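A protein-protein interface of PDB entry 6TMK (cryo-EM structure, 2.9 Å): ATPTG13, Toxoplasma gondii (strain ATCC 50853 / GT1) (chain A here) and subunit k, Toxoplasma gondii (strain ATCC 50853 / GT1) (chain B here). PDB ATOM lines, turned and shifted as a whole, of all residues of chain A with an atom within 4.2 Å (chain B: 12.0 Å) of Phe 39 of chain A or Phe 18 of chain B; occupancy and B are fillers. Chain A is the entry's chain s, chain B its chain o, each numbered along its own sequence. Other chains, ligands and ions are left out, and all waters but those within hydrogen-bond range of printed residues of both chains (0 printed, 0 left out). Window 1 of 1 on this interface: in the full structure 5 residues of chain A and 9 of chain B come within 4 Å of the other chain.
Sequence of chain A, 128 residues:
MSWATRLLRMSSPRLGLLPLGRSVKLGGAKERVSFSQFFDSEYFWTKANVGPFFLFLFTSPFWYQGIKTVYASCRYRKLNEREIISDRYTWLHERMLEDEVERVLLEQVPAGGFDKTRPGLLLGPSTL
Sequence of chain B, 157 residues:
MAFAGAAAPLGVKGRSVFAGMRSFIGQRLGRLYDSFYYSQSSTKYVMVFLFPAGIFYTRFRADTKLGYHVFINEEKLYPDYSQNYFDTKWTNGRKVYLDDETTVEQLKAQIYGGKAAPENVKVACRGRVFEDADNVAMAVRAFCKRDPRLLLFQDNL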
ATOM      1  N   PHE A  35      -9.716  -1.436  11.936  1.00  0.00           N
ATOM      2  CA  PHE A  35      -8.681  -2.094  11.145  1.00  0.00           C
ATOM      3  C   PHE A  35      -8.835  -1.777   9.662  1.00  0.00           C
ATOM      4  O   PHE A  35      -7.870  -1.391   8.987  1.00  0.00           O
ATOM      5  CB  PHE A  35      -8.765  -3.601  11.385  1.00  0.00           C
ATOM      6  CG  PHE A  35      -7.570  -4.371  10.910  1.00  0.00           C
ATOM      7  CD1 PHE A  35      -6.501  -4.601  11.754  1.00  0.00           C
ATOM      8  CD2 PHE A  35      -7.531  -4.890   9.627  1.00  0.00           C
ATOM      9  CE1 PHE A  35      -5.405  -5.321  11.325  1.00  0.00           C
ATOM     10  CE2 PHE A  35      -6.438  -5.609   9.191  1.00  0.00           C
ATOM     11  CZ  PHE A  35      -5.374  -5.825  10.040  1.00  0.00           C
ATOM     12  N   SER A  36     -10.054  -1.925   9.141  1.00  0.00           N
ATOM     13  CA  SER A  36     -10.294  -1.732   7.716  1.00  0.00           C
ATOM     14  C   SER A  36     -10.001  -0.300   7.295  1.00  0.00           C
ATOM     15  O   SER A  36      -9.209  -0.056   6.377  1.00  0.00           O
ATOM     16  CB  SER A  36     -11.738  -2.106   7.379  1.00  0.00           C
ATOM     17  OG  SER A  36     -11.907  -3.513   7.338  1.00  0.00           O
ATOM     18  N   GLN A  37     -10.646   0.667   7.946  1.00  0.00           N
ATOM     19  CA  GLN A  37     -10.460   2.056   7.551  1.00  0.00           C
ATOM     20  C   GLN A  37      -9.064   2.566   7.874  1.00  0.00           C
ATOM     21  O   GLN A  37      -8.640   3.575   7.301  1.00  0.00           O
ATOM     22  CB  GLN A  37     -11.506   2.934   8.233  1.00  0.00           C
ATOM     23  CG  GLN A  37     -11.248   3.161   9.709  1.00  0.00           C
ATOM     24  CD  GLN A  37     -12.513   3.486  10.480  1.00  0.00           C
ATOM     25  OE1 GLN A  37     -13.582   2.944  10.200  1.00  0.00           O
ATOM     26  NE2 GLN A  37     -12.394   4.368  11.465  1.00  0.00           N
ATOM     27  N   PHE A  38      -8.339   1.900   8.773  1.00  0.00           N
ATOM     28  CA  PHE A  38      -6.930   2.221   8.962  1.00  0.00           C
ATOM     29  C   PHE A  38      -6.101   1.760   7.774  1.00  0.00           C
ATOM     30  O   PHE A  38      -5.322   2.534   7.208  1.00  0.00           O
ATOM     31  CB  PHE A  38      -6.397   1.589  10.243  1.00  0.00           C
ATOM     32  CG  PHE A  38      -4.936   1.835  10.459  1.00  0.00           C
ATOM     33  CD1 PHE A  38      -4.486   3.048  10.939  1.00  0.00           C
ATOM     34  CD2 PHE A  38      -4.011   0.855  10.167  1.00  0.00           C
ATOM     35  CE1 PHE A  38      -3.142   3.274  11.130  1.00  0.00           C
ATOM     36  CE2 PHE A  38      -2.669   1.077  10.356  1.00  0.00           C
ATOM     37  CZ  PHE A  38      -2.234   2.288  10.839  1.00  0.00           C
ATOM     38  N   PHE A  39      -6.259   0.502   7.383  1.00  0.00           N
ATOM     39  CA  PHE A  39      -5.473  -0.063   6.298  1.00  0.00           C
ATOM     40  C   PHE A  39      -6.014   0.284   4.921  1.00  0.00           C
ATOM     41  O   PHE A  39      -5.495  -0.226   3.923  1.00  0.00           O
ATOM     42  CB  PHE A  39      -5.375  -1.576   6.463  1.00  0.00           C
ATOM     43  CG  PHE A  39      -4.362  -1.995   7.479  1.00  0.00           C
ATOM     44  CD1 PHE A  39      -3.013  -1.898   7.207  1.00  0.00           C
ATOM     45  CD2 PHE A  39      -4.755  -2.469   8.715  1.00  0.00           C
ATOM     46  CE1 PHE A  39      -2.079  -2.272   8.140  1.00  0.00           C
ATOM     47  CE2 PHE A  39      -3.823  -2.845   9.651  1.00  0.00           C
ATOM     48  CZ  PHE A  39      -2.482  -2.748   9.363  1.00  0.00           C
ATOM     49  N   ASP A  40      -7.035   1.129   4.838  1.00  0.00           N
ATOM     50  CA  ASP A  40      -7.403   1.709   3.556  1.00  0.00           C
ATOM     51  C   ASP A  40      -6.291   2.629   3.068  1.00  0.00           C
ATOM     52  O   ASP A  40      -5.675   3.358   3.849  1.00  0.00           O
ATOM     53  CB  ASP A  40      -8.713   2.479   3.678  1.00  0.00           C
ATOM     54  CG  ASP A  40      -9.164   3.074   2.362  1.00  0.00           C
ATOM     55  OD1 ASP A  40      -9.031   4.304   2.187  1.00  0.00           O
ATOM     56  OD2 ASP A  40      -9.649   2.313   1.500  1.00  0.00           O
ATOM     57  N   SER A  41      -6.041   2.593   1.760  1.00  0.00           N
ATOM     58  CA  SER A  41      -4.837   3.208   1.211  1.00  0.00           C
ATOM     59  C   SER A  41      -4.821   4.711   1.448  1.00  0.00           C
ATOM     60  O   SER A  41      -3.800   5.278   1.857  1.00  0.00           O
ATOM     61  CB  SER A  41      -4.735   2.901  -0.280  1.00  0.00           C
ATOM     62  OG  SER A  41      -4.490   1.527  -0.496  1.00  0.00           O
ATOM     63  N   PHE A  53       3.415   1.632  13.704  1.00  0.00           N
ATOM     64  CA  PHE A  53       3.270   0.410  12.926  1.00  0.00           C
ATOM     65  C   PHE A  53       4.596   0.003  12.299  1.00  0.00           C
ATOM     66  O   PHE A  53       5.039  -1.143  12.440  1.00  0.00           O
ATOM     67  CB  PHE A  53       2.199   0.597  11.853  1.00  0.00           C
ATOM     68  CG  PHE A  53       2.083  -0.560  10.913  1.00  0.00           C
ATOM     69  CD1 PHE A  53       2.455  -0.438   9.590  1.00  0.00           C
ATOM     70  CD2 PHE A  53       1.607  -1.777  11.357  1.00  0.00           C
ATOM     71  CE1 PHE A  53       2.351  -1.506   8.730  1.00  0.00           C
ATOM     72  CE2 PHE A  53       1.500  -2.846  10.500  1.00  0.00           C
ATOM     73  CZ  PHE A  53       1.874  -2.710   9.183  1.00  0.00           C
ATOM     74  N   LEU B  10      -1.570   9.875  -3.299  1.00  0.00           N
ATOM     75  CA  LEU B  10      -1.177   8.561  -2.815  1.00  0.00           C
ATOM     76  C   LEU B  10      -2.404   7.799  -2.341  1.00  0.00           C
ATOM     77  O   LEU B  10      -3.244   8.345  -1.618  1.00  0.00           O
ATOM     78  CB  LEU B  10      -0.166   8.679  -1.679  1.00  0.00           C
ATOM     79  CG  LEU B  10       1.012   9.618  -1.907  1.00  0.00           C
ATOM     80  CD1 LEU B  10       1.952   9.530  -0.735  1.00  0.00           C
ATOM     81  CD2 LEU B  10       1.726   9.273  -3.194  1.00  0.00           C
ATOM     82  N   GLY B  11      -2.502   6.543  -2.753  1.00  0.00           N
ATOM     83  CA  GLY B  11      -3.597   5.698  -2.336  1.00  0.00           C
ATOM     84  C   GLY B  11      -4.909   6.028  -3.008  1.00  0.00           C
ATOM     85  O   GLY B  11      -5.118   7.148  -3.481  1.00  0.00           O
ATOM     86  N   VAL B  12      -5.803   5.045  -3.051  1.00  0.00           N
ATOM     87  CA  VAL B  12      -7.146   5.212  -3.580  1.00  0.00           C
ATOM     88  C   VAL B  12      -8.127   4.610  -2.588  1.00  0.00           C
ATOM     89  O   VAL B  12      -7.811   3.650  -1.878  1.00  0.00           O
ATOM     90  CB  VAL B  12      -7.303   4.557  -4.967  1.00  0.00           C
ATOM     91  CG1 VAL B  12      -7.146   3.056  -4.862  1.00  0.00           C
ATOM     92  CG2 VAL B  12      -8.644   4.914  -5.567  1.00  0.00           C
ATOM     93  N   LYS B  13      -9.325   5.180  -2.541  1.00  0.00           N
ATOM     94  CA  LYS B  13     -10.329   4.737  -1.588  1.00  0.00           C
ATOM     95  C   LYS B  13     -10.961   3.435  -2.058  1.00  0.00           C
ATOM     96  O   LYS B  13     -11.170   3.225  -3.256  1.00  0.00           O
ATOM     97  CB  LYS B  13     -11.403   5.806  -1.403  1.00  0.00           C
ATOM     98  CG  LYS B  13     -12.287   5.574  -0.194  1.00  0.00           C
ATOM     99  CD  LYS B  13     -13.075   6.815   0.167  1.00  0.00           C
ATOM    100  CE  LYS B  13     -14.110   7.143  -0.890  1.00  0.00           C
ATOM    101  NZ  LYS B  13     -14.990   8.261  -0.462  1.00  0.00           N
ATOM    102  N   GLY B  14     -11.264   2.560  -1.104  1.00  0.00           N
ATOM    103  CA  GLY B  14     -11.792   1.251  -1.404  1.00  0.00           C
ATOM    104  C   GLY B  14     -10.749   0.200  -1.702  1.00  0.00           C
ATOM    105  O   GLY B  14     -11.097  -0.985  -1.794  1.00  0.00           O
ATOM    106  N   ARG B  15      -9.488   0.587  -1.853  1.00  0.00           N
ATOM    107  CA  ARG B  15      -8.408  -0.339  -2.148  1.00  0.00           C
ATOM    108  C   ARG B  15      -7.513  -0.472  -0.926  1.00  0.00           C
ATOM    109  O   ARG B  15      -7.336   0.476  -0.157  1.00  0.00           O
ATOM    110  CB  ARG B  15      -7.581   0.129  -3.345  1.00  0.00           C
ATOM    111  CG  ARG B  15      -6.608  -0.917  -3.848  1.00  0.00           C
ATOM    112  CD  ARG B  15      -6.081  -0.589  -5.224  1.00  0.00           C
ATOM    113  NE  ARG B  15      -5.459  -1.749  -5.857  1.00  0.00           N
ATOM    114  CZ  ARG B  15      -4.177  -1.846  -6.200  1.00  0.00           C
ATOM    115  NH1 ARG B  15      -3.741  -2.957  -6.770  1.00  0.00           N
ATOM    116  NH2 ARG B  15      -3.322  -0.858  -5.970  1.00  0.00           N
ATOM    117  N   SER B  16      -6.950  -1.661  -0.753  1.00  0.00           N
ATOM    118  CA  SER B  16      -6.134  -1.980   0.404  1.00  0.00           C
ATOM    119  C   SER B  16      -4.663  -2.114   0.028  1.00  0.00           C
ATOM    120  O   SER B  16      -4.310  -2.496  -1.096  1.00  0.00           O
ATOM    121  CB  SER B  16      -6.614  -3.270   1.068  1.00  0.00           C
ATOM    122  OG  SER B  16      -5.949  -3.484   2.298  1.00  0.00           O
ATOM    123  N   VAL B  17      -3.810  -1.809   1.005  1.00  0.00           N
ATOM    124  CA  VAL B  17      -2.372  -1.930   0.808  1.00  0.00           C
ATOM    125  C   VAL B  17      -1.993  -3.379   0.559  1.00  0.00           C
ATOM    126  O   VAL B  17      -1.012  -3.666  -0.134  1.00  0.00           O
ATOM    127  CB  VAL B  17      -1.631  -1.349   2.027  1.00  0.00           C
ATOM    128  CG1 VAL B  17      -2.103   0.055   2.312  1.00  0.00           C
ATOM    129  CG2 VAL B  17      -1.853  -2.215   3.238  1.00  0.00           C
ATOM    130  N   PHE B  18      -2.777  -4.315   1.087  1.00  0.00           N
ATOM    131  CA  PHE B  18      -2.517  -5.726   0.835  1.00  0.00           C
ATOM    132  C   PHE B  18      -2.846  -6.081  -0.609  1.00  0.00           C
ATOM    133  O   PHE B  18      -2.130  -6.864  -1.248  1.00  0.00           O
ATOM    134  CB  PHE B  18      -3.330  -6.573   1.806  1.00  0.00           C
ATOM    135  CG  PHE B  18      -3.229  -6.109   3.226  1.00  0.00           C
ATOM    136  CD1 PHE B  18      -2.010  -6.081   3.874  1.00  0.00           C
ATOM    137  CD2 PHE B  18      -4.352  -5.683   3.909  1.00  0.00           C
ATOM    138  CE1 PHE B  18      -1.915  -5.648   5.176  1.00  0.00           C
ATOM    139  CE2 PHE B  18      -4.261  -5.250   5.211  1.00  0.00           C
ATOM    140  CZ  PHE B  18      -3.042  -5.232   5.845  1.00  0.00           C
ATOM    141  N   ALA B  19      -3.921  -5.503  -1.142  1.00  0.00           N
ATOM    142  CA  ALA B  19      -4.228  -5.677  -2.553  1.00  0.00           C
ATOM    143  C   ALA B  19      -3.117  -5.105  -3.417  1.00  0.00           C
ATOM    144  O   ALA B  19      -2.742  -5.695  -4.437  1.00  0.00           O
ATOM    145  CB  ALA B  19      -5.558  -5.009  -2.882  1.00  0.00           C
ATOM    146  N   GLY B  20      -2.569  -3.958  -3.019  1.00  0.00           N
ATOM    147  CA  GLY B  20      -1.457  -3.401  -3.765  1.00  0.00           C
ATOM    148  C   GLY B  20      -0.214  -4.268  -3.692  1.00  0.00           C
ATOM    149  O   GLY B  20       0.525  -4.392  -4.673  1.00  0.00           O
ATOM    150  N   MET B  21       0.036  -4.876  -2.534  1.00  0.00           N
ATOM    151  CA  MET B  21       1.135  -5.827  -2.420  1.00  0.00           C
ATOM    152  C   MET B  21       0.951  -7.005  -3.368  1.00  0.00           C
ATOM    153  O   MET B  21       1.897  -7.434  -4.037  1.00  0.00           O
ATOM    154  CB  MET B  21       1.240  -6.330  -0.982  1.00  0.00           C
ATOM    155  CG  MET B  21       1.889  -5.368  -0.012  1.00  0.00           C
ATOM    156  SD  MET B  21       2.563  -6.241   1.413  1.00  0.00           S
ATOM    157  CE  MET B  21       1.070  -6.638   2.319  1.00  0.00           C
ATOM    158  N   ARG B  22      -0.259  -7.568  -3.410  1.00  0.00           N
ATOM    159  CA  ARG B  22      -0.527  -8.663  -4.336  1.00  0.00           C
ATOM    160  C   ARG B  22      -0.293  -8.233  -5.780  1.00  0.00           C
ATOM    161  O   ARG B  22       0.320  -8.967  -6.567  1.00  0.00           O
ATOM    162  CB  ARG B  22      -1.954  -9.173  -4.139  1.00  0.00           C
ATOM    163  CG  ARG B  22      -2.344 -10.326  -5.049  1.00  0.00           C
ATOM    164  CD  ARG B  22      -3.755 -10.806  -4.764  1.00  0.00           C
ATOM    165  NE  ARG B  22      -4.105 -11.982  -5.557  1.00  0.00           N
ATOM    166  CZ  ARG B  22      -5.298 -12.569  -5.538  1.00  0.00           C
ATOM    167  NH1 ARG B  22      -5.526 -13.634  -6.295  1.00  0.00           N
ATOM    168  NH2 ARG B  22      -6.265 -12.093  -4.763  1.00  0.00           N
ATOM    169  N   SER B  23      -0.776  -7.044  -6.139  1.00  0.00           N
ATOM    170  CA  SER B  23      -0.512  -6.481  -7.460  1.00  0.00           C
ATOM    171  C   SER B  23       0.982  -6.452  -7.754  1.00  0.00           C
ATOM    172  O   SER B  23       1.432  -6.880  -8.825  1.00  0.00           O
ATOM    173  CB  SER B  23      -1.104  -5.079  -7.549  1.00  0.00           C
ATOM    174  OG  SER B  23      -0.168  -4.114  -7.107  1.00  0.00           O
ATOM    175  N   PHE B  24       1.761  -5.908  -6.821  1.00  0.00           N
ATOM    176  CA  PHE B  24       3.191  -5.748  -7.047  1.00  0.00           C
ATOM    177  C   PHE B  24       3.875  -7.095  -7.215  1.00  0.00           C
ATOM    178  O   PHE B  24       4.746  -7.257  -8.079  1.00  0.00           O
ATOM    179  CB  PHE B  24       3.807  -4.984  -5.878  1.00  0.00           C
ATOM    180  CG  PHE B  24       5.248  -4.646  -6.065  1.00  0.00           C
ATOM    181  CD1 PHE B  24       5.646  -3.764  -7.048  1.00  0.00           C
ATOM    182  CD2 PHE B  24       6.210  -5.224  -5.258  1.00  0.00           C
ATOM    183  CE1 PHE B  24       6.976  -3.461  -7.219  1.00  0.00           C
ATOM    184  CE2 PHE B  24       7.536  -4.928  -5.426  1.00  0.00           C
ATOM    185  CZ  PHE B  24       7.924  -4.043  -6.403  1.00  0.00           C
ATOM    186  N   ILE B  25       3.512  -8.071  -6.385  1.00  0.00           N
ATOM    187  CA  ILE B  25       4.136  -9.383  -6.490  1.00  0.00           C
ATOM    188  C   ILE B  25       3.792 -10.024  -7.828  1.00  0.00           C
ATOM    189  O   ILE B  25       4.642 -10.657  -8.469  1.00  0.00           O
ATOM    190  CB  ILE B  25       3.708 -10.269  -5.307  1.00  0.00           C
ATOM    191  CG1 ILE B  25       4.208  -9.678  -3.988  1.00  0.00           C
ATOM    192  CG2 ILE B  25       4.238 -11.670  -5.474  1.00  0.00           C
ATOM    193  CD1 ILE B  25       5.703  -9.535  -3.885  1.00  0.00           C
ATOM    194  N   GLY B  26       2.545  -9.865  -8.275  1.00  0.00           N
ATOM    195  CA  GLY B  26       2.179 -10.352  -9.594  1.00  0.00           C
ATOM    196  C   GLY B  26       3.005  -9.720 -10.696  1.00  0.00           C
ATOM    197  O   GLY B  26       3.478 -10.406 -11.607  1.00  0.00           O
ATOM    198  N   GLN B  27       3.187  -8.402 -10.627  1.00  0.00           N
ATOM    199  CA  GLN B  27       4.006  -7.709 -11.615  1.00  0.00           C
ATOM    200  C   GLN B  27       5.422  -8.263 -11.631  1.00  0.00           C
ATOM    201  O   GLN B  27       5.979  -8.555 -12.698  1.00  0.00           O
ATOM    202  CB  GLN B  27       4.028  -6.213 -11.325  1.00  0.00           C
ATOM    203  CG  GLN B  27       2.707  -5.510 -11.539  1.00  0.00           C
ATOM    204  CD  GLN B  27       2.699  -4.119 -10.943  1.00  0.00           C
ATOM    205  OE1 GLN B  27       3.747  -3.579 -10.590  1.00  0.00           O
ATOM    206  NE2 GLN B  27       1.518  -3.529 -10.832  1.00  0.00           N
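O of Phe 39 of chain A touches OG of Ser 16 of chain B, 3.7 Å away.
O of Phe 39 of chain A touches N of Val 17 of chain B, at 3.7 Å.
Phe 18 of chain B touches Phe 39 of chain A (CZ to CD1, 3.6 Å).
OD2 of Asp 40 of chain A touches C of Lys 13 of chain B (3.95 Å).
Ser 41 of chain A touches Gly 11 of chain B.
Val 12 of chain B touches Ser 41 of chain A (O to CB, 3.5 Å).
Ser 41 of chain A touches Ser 16 of chain B.
Ser 41 of chain A touches Val 17 of chain B.
O of Arg 15 of chain B lies within hydrogen-bond range of OG of Ser 41 of chain A, at 3.1 Å.
The side-chain carboxylate (OD2) of Asp 40 of chain A lies close to the backbone carbonyl oxygen (O) of Arg 15 of chain B, 3.4 Å away.
N of Gly 14 of chain B sits at hydrogen-bond distance from OD2 of Asp 40 of chain A, at 3.1 Å.
Of the 18 printed residues of chain B, 8 touch a printed residue of chain A.
Printed residues of chain B that touch a printed residue of chain A: Gly 11, Val 12, Lys 13, Gly 14, Arg 15, Ser 16, Val 17 and Phe 18.
Hydrophobic or aromatic side chains of chain B within 4 Å of the printed part of chain A: Val 17 and Phe 18.
Among the printed residues, 11 pairs touch across the chains.
The backbone NH of Phe 18 of chain B sits close to the side-chain hydroxyl of Ser 16 of chain B (3.5 Å).
Of the printed residues of chain B, Phe 39 of chain A touches Ser 16 (3.7 Å), Val 17 (3.7 Å) and Phe 18 (3.6 Å).
Phe 18 of chain B touches just one residue of chain A: Phe 39 (3.6 Å).
No residue of chain B comes within 4 Å of Phe 35 of chain A.
No residue of chain B comes within 4 Å of Phe 38 of chain A.
Printed residues of chain B within 4 Å of Asp 40 of chain A: Lys 13 (3.95 Å), Gly 14 (3.1 Å) and Arg 15 (3.4 Å).
Ser 41 of chain A touches just these residues of chain B: Gly 11, Val 12, Arg 15, Ser 16 and Val 17.
Printed residues of chain A within 4 Å of Arg 15 of chain B: Asp 40 and Ser 41.
Of the printed residues of chain A, Val 12 of chain B touches Ser 41.
Of the printed residues of chain A, Lys 13 of chain B touches Asp 40 (3.95 Å).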
